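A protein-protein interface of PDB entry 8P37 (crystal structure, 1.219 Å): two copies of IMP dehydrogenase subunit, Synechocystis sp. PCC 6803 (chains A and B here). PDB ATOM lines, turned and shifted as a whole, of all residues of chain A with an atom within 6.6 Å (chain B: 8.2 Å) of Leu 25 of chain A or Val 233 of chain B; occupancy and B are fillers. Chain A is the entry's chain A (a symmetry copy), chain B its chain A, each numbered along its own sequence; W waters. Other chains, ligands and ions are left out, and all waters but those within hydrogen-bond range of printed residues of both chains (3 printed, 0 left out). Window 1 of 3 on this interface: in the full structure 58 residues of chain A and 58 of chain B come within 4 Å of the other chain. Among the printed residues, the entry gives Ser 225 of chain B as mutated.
O of Gly 232 of chain B touches CA of Ala 24 of chain A, 3.7 Å away.
Leu 25 of chain A touches Val 233 of chain B.
Val 26 of chain A touches Thr 200 of chain B.
Val 26 of chain A touches Val 235 of chain B.
Ile 219 of chain B touches Pro 27 of chain A.
Gly 232 of chain B touches Gly 271 of chain A.
Cys 274 of chain A touches Leu 231 of chain B.
Val 166 of chain B touches Thr 353 of chain A.
No position is printed for both chains.
Of the 27 pairs that touch across the chains among the printed residues, none has its exchanged pair printed and touching as well.
Of the printed residues of chain A, Val 233 of chain B touches Leu 25, Ser 350, Thr 353 and Leu 354.
Ala 24 of chain A touches just these residues of chain B: Gly 232 and Gly 234.
Of the printed residues of chain B, Thr 353 of chain A touches Val 166 and Val 233.
Printed residues of chain A within 4 Å of Val 166 of chain B: Thr 353.
Ile 23 of chain A touches none of the printed residues of chain B.
The nearest printed residue of chain A that does not touch Val 233 of chain B is Pro 27 of chain A (4.2 Å).
O of Ala 278 of chain A lies within hydrogen-bond range of NZ of Lys 12 of chain B (2.8 Å).
O of Val 365 of chain A sits at hydrogen-bond distance from NZ of Lys 12 of chain B (2.8 Å).
NH1 of Arg 228 of chain B sits close to O of Leu 373 of chain A (3.3 Å).
The backbone NH (N) of Gly 271 of chain A is in hydrogen-bond range of the backbone carbonyl oxygen (O) of Gly 229 of chain B, 3.0 Å away.
The backbone carbonyl oxygen of Val 230 of chain B sits at hydrogen-bond distance from the backbone NH of Gly 271 of chain A (3.1 Å).
The backbone carbonyl oxygen (O) of Leu 231 of chain B sits at hydrogen-bond distance from the side-chain hydroxyl (OG) of Ser 350 of chain A (2.8 Å).
The backbone NH of Leu 25 of chain A sits at hydrogen-bond distance from the backbone carbonyl oxygen of Gly 232 of chain B.
The backbone carbonyl oxygen (O) of Leu 25 of chain A sits at hydrogen-bond distance from the backbone NH (N) of Gly 234 of chain B (3.0 Å).
Printed residues of chain B that touch a printed residue of chain A: Ile 8, Lys 12, Val 166, Val 199, Thr 200, Ile 219, Arg 228, Gly 229, Val 230, Leu 231, Gly 232, Val 233, Gly 234 and Val 235.
Hydrophobic or aromatic side chains of chain B within 4 Å of the printed part of chain A: Ile 8, Val 166, Val 199, Ile 219, Leu 231, Val 233 and Val 235.
Along chain B the printed residues that touch a printed residue of chain A span positions 8 to 235.
Hydrophobic or aromatic side chains of chain A within 4 Å of the printed part of chain B: Ala 24, Leu 25, Val 26, Pro 27, Leu 354, Val 367 and Leu 373.
Among the printed residues, 27 pairs touch across the chains.
Among the printed residues, no Asp or Glu carboxylate lies within 4 Å of a Lys or Arg side-chain nitrogen of the other chain.
Water W3 lies within hydrogen-bond range of the backbone carbonyl oxygen of Leu 373 of chain A (2.4 Å) and the guanidinium group of Arg 228 of chain B (2.9 Å).
Water W1 bridges OG1 of Thr 200 of chain B (2.6 Å) and O of Pro 27 of chain A (3.3 Å).
Water W2 lies within hydrogen-bond range of O of Arg 228 of chain B (2.8 Å) and NZ of Lys 275 of chain A (2.9 Å).
The backbone carbonyl oxygen of Ile 219 of chain B is in hydrogen-bond range of the guanidinium group of Arg 228 of chain B, 2.9 Å away.
The guanidinium group of Arg 228 of chain B sits close to the backbone carbonyl oxygen of Gly 220 of chain B (3.3 Å).
The side-chain sulfur (SG) of Cys 274 of chain A sits close to the side-chain hydroxyl (OG) of Ser 350 of chain A.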
ATOM      1  N   ILE A  23     -21.373 -38.993  -4.841  1.00  0.00           N
ATOM      2  CA  ILE A  23     -20.410 -38.034  -4.293  1.00  0.00           C
ATOM      3  C   ILE A  23     -20.791 -36.602  -4.613  1.00  0.00           C
ATOM      4  O   ILE A  23     -21.654 -36.344  -5.481  1.00  0.00           O
ATOM      5  CB  ILE A  23     -18.974 -38.372  -4.752  1.00  0.00           C
ATOM      6  CG1 ILE A  23     -18.776 -38.027  -6.245  1.00  0.00           C
ATOM      7  CG2 ILE A  23     -18.576 -39.822  -4.450  1.00  0.00           C
ATOM      8  CD1 ILE A  23     -17.297 -38.006  -6.628  1.00  0.00           C
ATOM      9  N   ALA A  24     -20.165 -35.674  -3.908  1.00  0.00           N
ATOM     10  CA  ALA A  24     -20.408 -34.261  -4.114  1.00  0.00           C
ATOM     11  C   ALA A  24     -19.187 -33.477  -3.765  1.00  0.00           C
ATOM     12  O   ALA A  24     -18.358 -33.886  -2.956  1.00  0.00           O
ATOM     13  CB  ALA A  24     -21.582 -33.802  -3.264  1.00  0.00           C
ATOM     14  N   LEU A  25     -19.077 -32.287  -4.314  1.00  0.00           N
ATOM     15  CA  LEU A  25     -17.889 -31.443  -4.164  1.00  0.00           C
ATOM     16  C   LEU A  25     -18.104 -30.299  -3.179  1.00  0.00           C
ATOM     17  O   LEU A  25     -19.153 -29.652  -3.147  1.00  0.00           O
ATOM     18  CB  LEU A  25     -17.450 -30.874  -5.521  1.00  0.00           C
ATOM     19  CG  LEU A  25     -17.386 -31.910  -6.644  1.00  0.00           C
ATOM     20  CD1 LEU A  25     -16.858 -31.275  -7.901  1.00  0.00           C
ATOM     21  CD2 LEU A  25     -16.548 -33.108  -6.254  1.00  0.00           C
ATOM     22  N   VAL A  26     -17.113 -30.072  -2.321  1.00  0.00           N
ATOM     23  CA  VAL A  26     -17.239 -29.134  -1.215  1.00  0.00           C
ATOM     24  C   VAL A  26     -16.425 -27.889  -1.471  1.00  0.00           C
ATOM     25  O   VAL A  26     -15.227 -27.968  -1.783  1.00  0.00           O
ATOM     26  CB  VAL A  26     -16.763 -29.791   0.093  1.00  0.00           C
ATOM     27  CG1 VAL A  26     -16.977 -28.889   1.299  1.00  0.00           C
ATOM     28  CG2 VAL A  26     -17.455 -31.137   0.333  1.00  0.00           C
ATOM     29  N   PRO A  27     -16.994 -26.684  -1.276  1.00  0.00           N
ATOM     30  CA  PRO A  27     -16.203 -25.457  -1.456  1.00  0.00           C
ATOM     31  C   PRO A  27     -15.011 -25.418  -0.511  1.00  0.00           C
ATOM     32  O   PRO A  27     -14.979 -26.030   0.570  1.00  0.00           O
ATOM     33  CB  PRO A  27     -17.173 -24.353  -1.062  1.00  0.00           C
ATOM     34  CG  PRO A  27     -18.512 -24.896  -1.284  1.00  0.00           C
ATOM     35  CD  PRO A  27     -18.420 -26.363  -1.003  1.00  0.00           C
ATOM     36  N   GLY A 271     -21.970 -31.493 -13.981  1.00  0.00           N
ATOM     37  CA  GLY A 271     -21.667 -31.915 -12.625  1.00  0.00           C
ATOM     38  C   GLY A 271     -20.987 -33.263 -12.615  1.00  0.00           C
ATOM     39  O   GLY A 271     -20.046 -33.489 -11.851  1.00  0.00           O
ATOM     40  N   CYS A 274     -17.349 -32.695 -13.443  1.00  0.00           N
ATOM     41  CA  CYS A 274     -16.644 -32.116 -12.314  1.00  0.00           C
ATOM     42  C   CYS A 274     -16.341 -33.131 -11.240  1.00  0.00           C
ATOM     43  O   CYS A 274     -15.231 -33.121 -10.637  1.00  0.00           O
ATOM     44  CB  CYS A 274     -17.416 -30.916 -11.779  1.00  0.00           C
ATOM     45  SG  CYS A 274     -17.500 -29.558 -12.961  1.00  0.00           S
ATOM     46  N   LYS A 275     -17.291 -33.999 -10.970  1.00  0.00           N
ATOM     47  CA  LYS A 275     -17.100 -35.059  -9.974  1.00  0.00           C
ATOM     48  C   LYS A 275     -15.979 -35.999 -10.412  1.00  0.00           C
ATOM     49  O   LYS A 275     -15.159 -36.415  -9.561  1.00  0.00           O
ATOM     50  CB  LYS A 275     -18.411 -35.816  -9.757  1.00  0.00           C
ATOM     51  CG  LYS A 275     -19.494 -35.045  -9.029  1.00  0.00           C
ATOM     52  CD  LYS A 275     -20.820 -35.842  -9.218  1.00  0.00           C
ATOM     53  CE  LYS A 275     -21.954 -35.296  -8.489  1.00  0.00           C
ATOM     54  NZ  LYS A 275     -23.135 -36.072  -8.882  1.00  0.00           N
ATOM     55  N   CYS A 276     -15.876 -36.302 -11.690  1.00  0.00           N
ATOM     56  CA  CYS A 276     -14.773 -37.134 -12.203  1.00  0.00           C
ATOM     57  C   CYS A 276     -13.435 -36.470 -12.093  1.00  0.00           C
ATOM     58  O   CYS A 276     -12.453 -37.098 -11.636  1.00  0.00           O
ATOM     59  CB  CYS A 276     -15.064 -37.579 -13.625  1.00  0.00           C
ATOM     60  SG  CYS A 276     -16.411 -38.769 -13.750  1.00  0.00           S
ATOM     61  N   ALA A 278     -12.650 -34.187  -9.895  1.00  0.00           N
ATOM     62  CA  ALA A 278     -12.350 -34.104  -8.452  1.00  0.00           C
ATOM     63  C   ALA A 278     -11.803 -35.402  -7.896  1.00  0.00           C
ATOM     64  O   ALA A 278     -11.075 -35.381  -6.900  1.00  0.00           O
ATOM     65  CB  ALA A 278     -13.598 -33.713  -7.689  1.00  0.00           C
ATOM     66  N   CYS A 279     -12.065 -36.541  -8.555  1.00  0.00           N
ATOM     67  CA  CYS A 279     -11.513 -37.801  -8.124  1.00  0.00           C
ATOM     68  C   CYS A 279     -10.162 -38.118  -8.719  1.00  0.00           C
ATOM     69  O   CYS A 279      -9.587 -39.167  -8.351  1.00  0.00           O
ATOM     70  CB  CYS A 279     -12.506 -38.922  -8.360  1.00  0.00           C
ATOM     71  SG  CYS A 279     -13.990 -38.791  -7.348  1.00  0.00           S
ATOM     72  N   THR A 349     -17.414 -22.774 -14.059  1.00  0.00           N
ATOM     73  CA  THR A 349     -18.259 -22.247 -12.997  1.00  0.00           C
ATOM     74  C   THR A 349     -18.128 -23.088 -11.725  1.00  0.00           C
ATOM     75  O   THR A 349     -18.074 -22.543 -10.629  1.00  0.00           O
ATOM     76  CB  THR A 349     -19.699 -22.136 -13.469  1.00  0.00           C
ATOM     77  OG1 THR A 349     -19.722 -21.251 -14.595  1.00  0.00           O
ATOM     78  CG2 THR A 349     -20.603 -21.525 -12.427  1.00  0.00           C
ATOM     79  N   SER A 350     -18.010 -24.397 -11.862  1.00  0.00           N
ATOM     80  CA  SER A 350     -17.825 -25.286 -10.718  1.00  0.00           C
ATOM     81  C   SER A 350     -16.458 -25.058 -10.099  1.00  0.00           C
ATOM     82  O   SER A 350     -16.352 -24.818  -8.891  1.00  0.00           O
ATOM     83  CB  SER A 350     -17.955 -26.751 -11.162  1.00  0.00           C
ATOM     84  OG  SER A 350     -17.805 -27.612 -10.060  1.00  0.00           O
ATOM     85  N   MET A 351     -15.394 -25.021 -10.918  1.00  0.00           N
ATOM     86  CA  MET A 351     -14.045 -24.705 -10.428  1.00  0.00           C
ATOM     87  C   MET A 351     -14.051 -23.352  -9.699  1.00  0.00           C
ATOM     88  O   MET A 351     -13.502 -23.230  -8.616  1.00  0.00           O
ATOM     89  CB  MET A 351     -13.096 -24.631 -11.599  1.00  0.00           C
ATOM     90  CG  MET A 351     -12.790 -26.005 -12.230  1.00  0.00           C
ATOM     91  SD  MET A 351     -11.745 -25.906 -13.667  1.00  0.00           S
ATOM     92  CE  MET A 351     -10.201 -25.424 -12.923  1.00  0.00           C
ATOM     93  N   THR A 353     -16.549 -21.816  -8.134  1.00  0.00           N
ATOM     94  CA  THR A 353     -17.271 -21.996  -6.870  1.00  0.00           C
ATOM     95  C   THR A 353     -16.399 -22.644  -5.816  1.00  0.00           C
ATOM     96  O   THR A 353     -16.518 -22.337  -4.620  1.00  0.00           O
ATOM     97  CB  THR A 353     -18.515 -22.847  -7.101  1.00  0.00           C
ATOM     98  OG1 THR A 353     -19.329 -22.254  -8.120  1.00  0.00           O
ATOM     99  CG2 THR A 353     -19.317 -23.114  -5.889  1.00  0.00           C
ATOM    100  N   LEU A 354     -15.548 -23.581  -6.251  1.00  0.00           N
ATOM    101  CA  LEU A 354     -14.682 -24.342  -5.373  1.00  0.00           C
ATOM    102  C   LEU A 354     -13.337 -23.729  -5.113  1.00  0.00           C
ATOM    103  O   LEU A 354     -12.593 -24.221  -4.268  1.00  0.00           O
ATOM    104  CB  LEU A 354     -14.511 -25.738  -5.996  1.00  0.00           C
ATOM    105  CG  LEU A 354     -15.791 -26.570  -6.168  1.00  0.00           C
ATOM    106  CD1 LEU A 354     -15.557 -27.724  -7.082  1.00  0.00           C
ATOM    107  CD2 LEU A 354     -16.331 -27.041  -4.840  1.00  0.00           C
ATOM    108  N   MET A 362      -8.524 -28.738  -9.076  1.00  0.00           N
ATOM    109  CA  MET A 362      -9.848 -29.339  -9.092  1.00  0.00           C
ATOM    110  C   MET A 362      -9.773 -30.788  -8.603  1.00  0.00           C
ATOM    111  O   MET A 362     -10.652 -31.279  -7.866  1.00  0.00           O
ATOM    112  CB  MET A 362     -10.478 -29.251 -10.487  1.00  0.00           C
ATOM    113  CG  MET A 362     -11.904 -29.740 -10.558  1.00  0.00           C
ATOM    114  SD  MET A 362     -13.043 -28.752  -9.576  1.00  0.00           S
ATOM    115  CE  MET A 362     -14.522 -29.160 -10.429  1.00  0.00           C
ATOM    116  N   VAL A 365      -9.983 -31.012  -4.674  1.00  0.00           N
ATOM    117  CA  VAL A 365     -11.092 -30.482  -3.911  1.00  0.00           C
ATOM    118  C   VAL A 365     -11.606 -31.518  -2.934  1.00  0.00           C
ATOM    119  O   VAL A 365     -11.547 -32.733  -3.187  1.00  0.00           O
ATOM    120  CB  VAL A 365     -12.225 -29.934  -4.797  1.00  0.00           C
ATOM    121  CG1 VAL A 365     -11.747 -28.789  -5.684  1.00  0.00           C
ATOM    122  CG2 VAL A 365     -12.936 -31.008  -5.574  1.00  0.00           C
ATOM    123  N   ASP A 366     -12.164 -31.018  -1.831  1.00  0.00           N
ATOM    124  CA  ASP A 366     -12.762 -31.912  -0.852  1.00  0.00           C
ATOM    125  C   ASP A 366     -14.032 -32.503  -1.396  1.00  0.00           C
ATOM    126  O   ASP A 366     -14.799 -31.861  -2.113  1.00  0.00           O
ATOM    127  CB  ASP A 366     -13.020 -31.154   0.450  1.00  0.00           C
ATOM    128  CG  ASP A 366     -11.796 -30.718   1.227  1.00  0.00           C
ATOM    129  OD1 ASP A 366     -10.777 -31.390   1.139  1.00  0.00           O
ATOM    130  OD2 ASP A 366     -11.887 -29.707   1.952  1.00  0.00           O
ATOM    131  N   VAL A 367     -14.247 -33.770  -1.098  1.00  0.00           N
ATOM    132  CA  VAL A 367     -15.407 -34.538  -1.557  1.00  0.00           C
ATOM    133  C   VAL A 367     -16.161 -35.109  -0.366  1.00  0.00           C
ATOM    134  O   VAL A 367     -15.553 -35.490   0.628  1.00  0.00           O
ATOM    135  CB  VAL A 367     -14.953 -35.678  -2.501  1.00  0.00           C
ATOM    136  CG1 VAL A 367     -16.113 -36.619  -2.870  1.00  0.00           C
ATOM    137  CG2 VAL A 367     -14.323 -35.074  -3.749  1.00  0.00           C
ATOM    138  N   VAL A 368     -17.471 -35.160  -0.460  1.00  0.00           N
ATOM    139  CA  VAL A 368     -18.296 -35.862   0.507  1.00  0.00           C
ATOM    140  C   VAL A 368     -18.953 -37.037  -0.194  1.00  0.00           C
ATOM    141  O   VAL A 368     -19.283 -36.988  -1.392  1.00  0.00           O
ATOM    142  CB  VAL A 368     -19.357 -34.965   1.198  1.00  0.00           C
ATOM    143  CG1 VAL A 368     -18.714 -34.018   2.189  1.00  0.00           C
ATOM    144  CG2 VAL A 368     -20.237 -34.233   0.194  1.00  0.00           C
ATOM    145  N   LEU A 373     -27.362 -36.023  -2.711  1.00  0.00           N
ATOM    146  CA  LEU A 373     -27.098 -34.835  -3.524  1.00  0.00           C
ATOM    147  C   LEU A 373     -28.123 -34.659  -4.633  1.00  0.00           C
ATOM    148  O   LEU A 373     -28.585 -33.542  -4.859  1.00  0.00           O
ATOM    149  CB  LEU A 373     -25.721 -34.876  -4.146  1.00  0.00           C
ATOM    150  CG  LEU A 373     -25.280 -33.539  -4.776  1.00  0.00           C
ATOM    151  CD1 LEU A 373     -24.865 -32.549  -3.674  1.00  0.00           C
ATOM    152  CD2 LEU A 373     -24.186 -33.739  -5.794  1.00  0.00           C
ATOM    153  N   ILE B   8     -12.359 -43.144  -0.957  1.00  0.00           N
ATOM    154  CA  ILE B   8     -12.986 -43.313  -2.279  1.00  0.00           C
ATOM    155  C   ILE B   8     -12.067 -44.263  -3.061  1.00  0.00           C
ATOM    156  O   ILE B   8     -12.529 -45.221  -3.665  1.00  0.00           O
ATOM    157  CB  ILE B   8     -13.194 -41.986  -3.026  1.00  0.00           C
ATOM    158  CG1 ILE B   8     -14.331 -41.184  -2.349  1.00  0.00           C
ATOM    159  CG2 ILE B   8     -13.554 -42.274  -4.509  1.00  0.00           C
ATOM    160  CD1 ILE B   8     -14.488 -39.789  -2.796  1.00  0.00           C
ATOM    161  N   LYS B  12      -7.497 -40.633  -2.271  1.00  0.00           N
ATOM    162  CA  LYS B  12      -8.671 -39.766  -2.281  1.00  0.00           C
ATOM    163  C   LYS B  12      -9.601 -40.178  -1.168  1.00  0.00           C
ATOM    164  O   LYS B  12     -10.159 -41.282  -1.171  1.00  0.00           O
ATOM    165  CB  LYS B  12      -9.440 -39.793  -3.595  1.00  0.00           C
ATOM    166  CG  LYS B  12     -10.488 -38.680  -3.727  1.00  0.00           C
ATOM    167  CD  LYS B  12      -9.850 -37.318  -4.041  1.00  0.00           C
ATOM    168  CE  LYS B  12     -10.785 -36.151  -3.921  1.00  0.00           C
ATOM    169  NZ  LYS B  12     -10.108 -34.885  -4.337  1.00  0.00           N
ATOM    170  N   THR B 165     -24.847 -18.313  -4.776  1.00  0.00           N
ATOM    171  CA  THR B 165     -24.517 -19.731  -4.597  1.00  0.00           C
ATOM    172  C   THR B 165     -23.415 -19.883  -3.534  1.00  0.00           C
ATOM    173  O   THR B 165     -23.583 -20.669  -2.591  1.00  0.00           O
ATOM    174  CB  THR B 165     -24.060 -20.364  -5.909  1.00  0.00           C
ATOM    175  OG1 THR B 165     -25.033 -20.166  -6.913  1.00  0.00           O
ATOM    176  CG2 THR B 165     -23.759 -21.826  -5.725  1.00  0.00           C
ATOM    177  N   VAL B 166     -22.360 -19.062  -3.681  1.00  0.00           N
ATOM    178  CA  VAL B 166     -21.286 -18.847  -2.703  1.00  0.00           C
ATOM    179  C   VAL B 166     -21.042 -17.326  -2.583  1.00  0.00           C
ATOM    180  O   VAL B 166     -21.154 -16.589  -3.556  1.00  0.00           O
ATOM    181  CB  VAL B 166     -19.986 -19.598  -3.051  1.00  0.00           C
ATOM    182  CG1 VAL B 166     -20.145 -21.107  -2.881  1.00  0.00           C
ATOM    183  CG2 VAL B 166     -19.526 -19.281  -4.473  1.00  0.00           C
ATOM    184  N   VAL B 199     -21.697 -23.834   3.108  1.00  0.00           N
ATOM    185  CA  VAL B 199     -21.982 -25.181   3.626  1.00  0.00           C
ATOM    186  C   VAL B 199     -20.866 -25.686   4.518  1.00  0.00           C
ATOM    187  O   VAL B 199     -20.896 -26.867   4.880  1.00  0.00           O
ATOM    188  CB  VAL B 199     -22.246 -26.188   2.505  1.00  0.00           C
ATOM    189  CG1 VAL B 199     -23.525 -25.895   1.743  1.00  0.00           C
ATOM    190  CG2 VAL B 199     -21.079 -26.341   1.528  1.00  0.00           C
ATOM    191  N   THR B 200     -19.854 -24.894   4.832  1.00  0.00           N
ATOM    192  CA  THR B 200     -18.711 -25.366   5.633  1.00  0.00           C
ATOM    193  C   THR B 200     -18.489 -24.527   6.861  1.00  0.00           C
ATOM    194  O   THR B 200     -18.780 -23.316   6.920  1.00  0.00           O
ATOM    195  CB  THR B 200     -17.428 -25.419   4.797  1.00  0.00           C
ATOM    196  OG1 THR B 200     -17.031 -24.104   4.383  1.00  0.00           O
ATOM    197  CG2 THR B 200     -17.567 -26.312   3.593  1.00  0.00           C
ATOM    198  N   GLY B 218     -26.690 -23.566   2.551  1.00  0.00           N
ATOM    199  CA  GLY B 218     -27.274 -24.445   1.558  1.00  0.00           C
ATOM    200  C   GLY B 218     -26.806 -24.167   0.160  1.00  0.00           C
ATOM    201  O   GLY B 218     -26.868 -23.020  -0.314  1.00  0.00           O
ATOM    202  N   ILE B 219     -26.324 -25.195  -0.529  1.00  0.00           N
ATOM    203  CA  ILE B 219     -25.944 -25.106  -1.926  1.00  0.00           C
ATOM    204  C   ILE B 219     -26.685 -26.196  -2.654  1.00  0.00           C
ATOM    205  O   ILE B 219     -26.375 -27.371  -2.477  1.00  0.00           O
ATOM    206  CB  ILE B 219     -24.413 -25.174  -2.179  1.00  0.00           C
ATOM    207  CG1 ILE B 219     -23.708 -23.917  -1.580  1.00  0.00           C
ATOM    208  CG2 ILE B 219     -24.138 -25.245  -3.699  1.00  0.00           C
ATOM    209  CD1 ILE B 219     -22.224 -24.060  -1.450  1.00  0.00           C
ATOM    210  N   GLY B 220     -27.664 -25.821  -3.472  1.00  0.00           N
ATOM    211  CA  GLY B 220     -28.403 -26.764  -4.265  1.00  0.00           C
ATOM    212  C   GLY B 220     -29.516 -27.615  -3.698  1.00  0.00           C
ATOM    213  O   GLY B 220     -29.998 -28.420  -4.479  1.00  0.00           O
ATOM    214  N   PRO B 221     -29.963 -27.529  -2.414  1.00  0.00           N
ATOM    215  CA  PRO B 221     -31.097 -28.373  -2.008  1.00  0.00           C
ATOM    216  C   PRO B 221     -32.440 -27.937  -2.581  1.00  0.00           C
ATOM    217  O   PRO B 221     -33.408 -28.669  -2.425  1.00  0.00           O
ATOM    218  CB  PRO B 221     -31.070 -28.249  -0.497  1.00  0.00           C
ATOM    219  CG  PRO B 221     -30.603 -26.811  -0.252  1.00  0.00           C
ATOM    220  CD  PRO B 221     -29.527 -26.639  -1.322  1.00  0.00           C
ATOM    221  N   SER B 225     -33.857 -25.811  -7.880  1.00  0.00           N
ATOM    222  CA  SER B 225     -32.440 -25.727  -8.073  1.00  0.00           C
ATOM    223  C   SER B 225     -31.927 -26.795  -8.989  1.00  0.00           C
ATOM    224  O   SER B 225     -32.288 -27.955  -8.863  1.00  0.00           O
ATOM    225  CB  SER B 225     -31.767 -25.941  -6.727  1.00  0.00           C
ATOM    226  OG  SER B 225     -30.367 -26.145  -6.861  1.00  0.00           O
ATOM    227  N   THR B 226     -31.024 -26.403  -9.903  1.00  0.00           N
ATOM    228  CA  THR B 226     -30.302 -27.401 -10.719  1.00  0.00           C
ATOM    229  C   THR B 226     -28.792 -27.286 -10.540  1.00  0.00           C
ATOM    230  O   THR B 226     -28.070 -28.022 -11.209  1.00  0.00           O
ATOM    231  CB  THR B 226     -30.685 -27.396 -12.156  1.00  0.00           C
ATOM    232  OG1 THR B 226     -30.251 -26.169 -12.751  1.00  0.00           O
ATOM    233  CG2 THR B 226     -32.147 -27.552 -12.357  1.00  0.00           C
ATOM    234  N   SER B 227     -28.298 -26.478  -9.588  1.00  0.00           N
ATOM    235  CA  SER B 227     -26.851 -26.319  -9.390  1.00  0.00           C
ATOM    236  C   SER B 227     -26.081 -27.585  -9.115  1.00  0.00           C
ATOM    237  O   SER B 227     -24.946 -27.718  -9.561  1.00  0.00           O
ATOM    238  CB  SER B 227     -26.530 -25.327  -8.287  1.00  0.00           C
ATOM    239  OG  SER B 227     -27.001 -24.023  -8.606  1.00  0.00           O
ATOM    240  N   ARG B 228     -26.671 -28.539  -8.385  1.00  0.00           N
ATOM    241  CA  ARG B 228     -25.965 -29.758  -8.078  1.00  0.00           C
ATOM    242  C   ARG B 228     -25.738 -30.589  -9.346  1.00  0.00           C
ATOM    243  O   ARG B 228     -24.696 -31.192  -9.520  1.00  0.00           O
ATOM    244  CB  ARG B 228     -26.663 -30.552  -6.995  1.00  0.00           C
ATOM    245  CG  ARG B 228     -26.546 -29.931  -5.616  1.00  0.00           C
ATOM    246  CD  ARG B 228     -27.529 -30.502  -4.648  1.00  0.00           C
ATOM    247  NE  ARG B 228     -27.350 -29.944  -3.316  1.00  0.00           N
ATOM    248  CZ  ARG B 228     -27.895 -30.409  -2.202  1.00  0.00           C
ATOM    249  NH1 ARG B 228     -28.618 -31.526  -2.217  1.00  0.00           N
ATOM    250  NH2 ARG B 228     -27.667 -29.802  -1.044  1.00  0.00           N
ATOM    251  N   GLY B 229     -26.686 -30.593 -10.272  1.00  0.00           N
ATOM    252  CA  GLY B 229     -26.547 -31.281 -11.555  1.00  0.00           C
ATOM    253  C   GLY B 229     -25.608 -30.559 -12.490  1.00  0.00           C
ATOM    254  O   GLY B 229     -24.841 -31.187 -13.209  1.00  0.00           O
ATOM    255  N   VAL B 230     -25.640 -29.216 -12.473  1.00  0.00           N
ATOM    256  CA  VAL B 230     -24.785 -28.441 -13.380  1.00  0.00           C
ATOM    257  C   VAL B 230     -23.330 -28.424 -12.947  1.00  0.00           C
ATOM    258  O   VAL B 230     -22.428 -28.480 -13.791  1.00  0.00           O
ATOM    259  CB  VAL B 230     -25.319 -26.991 -13.511  1.00  0.00           C
ATOM    260  CG1 VAL B 230     -24.438 -26.129 -14.399  1.00  0.00           C
ATOM    261  CG2 VAL B 230     -26.750 -26.976 -14.057  1.00  0.00           C
ATOM    262  N   LEU B 231     -23.103 -28.374 -11.637  1.00  0.00           N
ATOM    263  CA  LEU B 231     -21.758 -28.157 -11.072  1.00  0.00           C
ATOM    264  C   LEU B 231     -21.187 -29.276 -10.259  1.00  0.00           C
ATOM    265  O   LEU B 231     -19.984 -29.326 -10.030  1.00  0.00           O
ATOM    266  CB  LEU B 231     -21.792 -26.876 -10.168  1.00  0.00           C
ATOM    267  CG  LEU B 231     -22.378 -25.639 -10.784  1.00  0.00           C
ATOM    268  CD1 LEU B 231     -22.366 -24.514  -9.763  1.00  0.00           C
ATOM    269  CD2 LEU B 231     -21.567 -25.206 -12.046  1.00  0.00           C
ATOM    270  N   GLY B 232     -22.033 -30.149  -9.700  1.00  0.00           N
ATOM    271  CA  GLY B 232     -21.579 -31.217  -8.811  1.00  0.00           C
ATOM    272  C   GLY B 232     -21.270 -30.765  -7.401  1.00  0.00           C
ATOM    273  O   GLY B 232     -20.750 -31.567  -6.618  1.00  0.00           O
ATOM    274  N   VAL B 233     -21.578 -29.499  -7.074  1.00  0.00           N
ATOM    275  CA  VAL B 233     -21.227 -28.889  -5.811  1.00  0.00           C
ATOM    276  C   VAL B 233     -22.377 -28.959  -4.832  1.00  0.00           C
ATOM    277  O   VAL B 233     -23.488 -28.600  -5.180  1.00  0.00           O
ATOM    278  CB  VAL B 233     -20.744 -27.423  -5.991  1.00  0.00           C
ATOM    279  CG1 VAL B 233     -20.390 -26.748  -4.653  1.00  0.00           C
ATOM    280  CG2 VAL B 233     -19.569 -27.380  -6.950  1.00  0.00           C
ATOM    281  N   GLY B 234     -22.081 -29.307  -3.580  1.00  0.00           N
ATOM    282  CA  GLY B 234     -23.061 -29.210  -2.519  1.00  0.00           C
ATOM    283  C   GLY B 234     -22.723 -30.112  -1.375  1.00  0.00           C
ATOM    284  O   GLY B 234     -22.035 -31.106  -1.548  1.00  0.00           O
ATOM    285  N   VAL B 235     -23.268 -29.806  -0.212  1.00  0.00           N
ATOM    286  CA  VAL B 235     -23.195 -30.663   0.959  1.00  0.00           C
ATOM    287  C   VAL B 235     -24.635 -30.831   1.406  1.00  0.00           C
ATOM    288  O   VAL B 235     -25.244 -29.815   1.747  1.00  0.00           O
ATOM    289  CB  VAL B 235     -22.286 -30.136   2.098  1.00  0.00           C
ATOM    290  CG1 VAL B 235     -22.455 -31.001   3.345  1.00  0.00           C
ATOM    291  CG2 VAL B 235     -20.799 -30.025   1.695  1.00  0.00           C
ATOM    292  N   PRO B 236     -25.176 -32.030   1.562  1.00  0.00           N
ATOM    293  CA  PRO B 236     -26.565 -32.186   2.054  1.00  0.00           C
ATOM    294  C   PRO B 236     -26.818 -31.448   3.369  1.00  0.00           C
ATOM    295  O   PRO B 236     -25.902 -31.286   4.210  1.00  0.00           O
ATOM    296  CB  PRO B 236     -26.718 -33.679   2.143  1.00  0.00           C
ATOM    297  CG  PRO B 236     -25.758 -34.260   1.143  1.00  0.00           C
ATOM    298  CD  PRO B 236     -24.592 -33.318   1.146  1.00  0.00           C
HETATM  299  O   HOH W   1     -14.631 -24.263   3.344  1.00  0.00           O
HETATM  300  O   HOH W   2     -23.934 -33.740 -10.417  1.00  0.00           O
HETATM  301  O   HOH W   3     -30.463 -32.086  -4.357  1.00  0.00           O
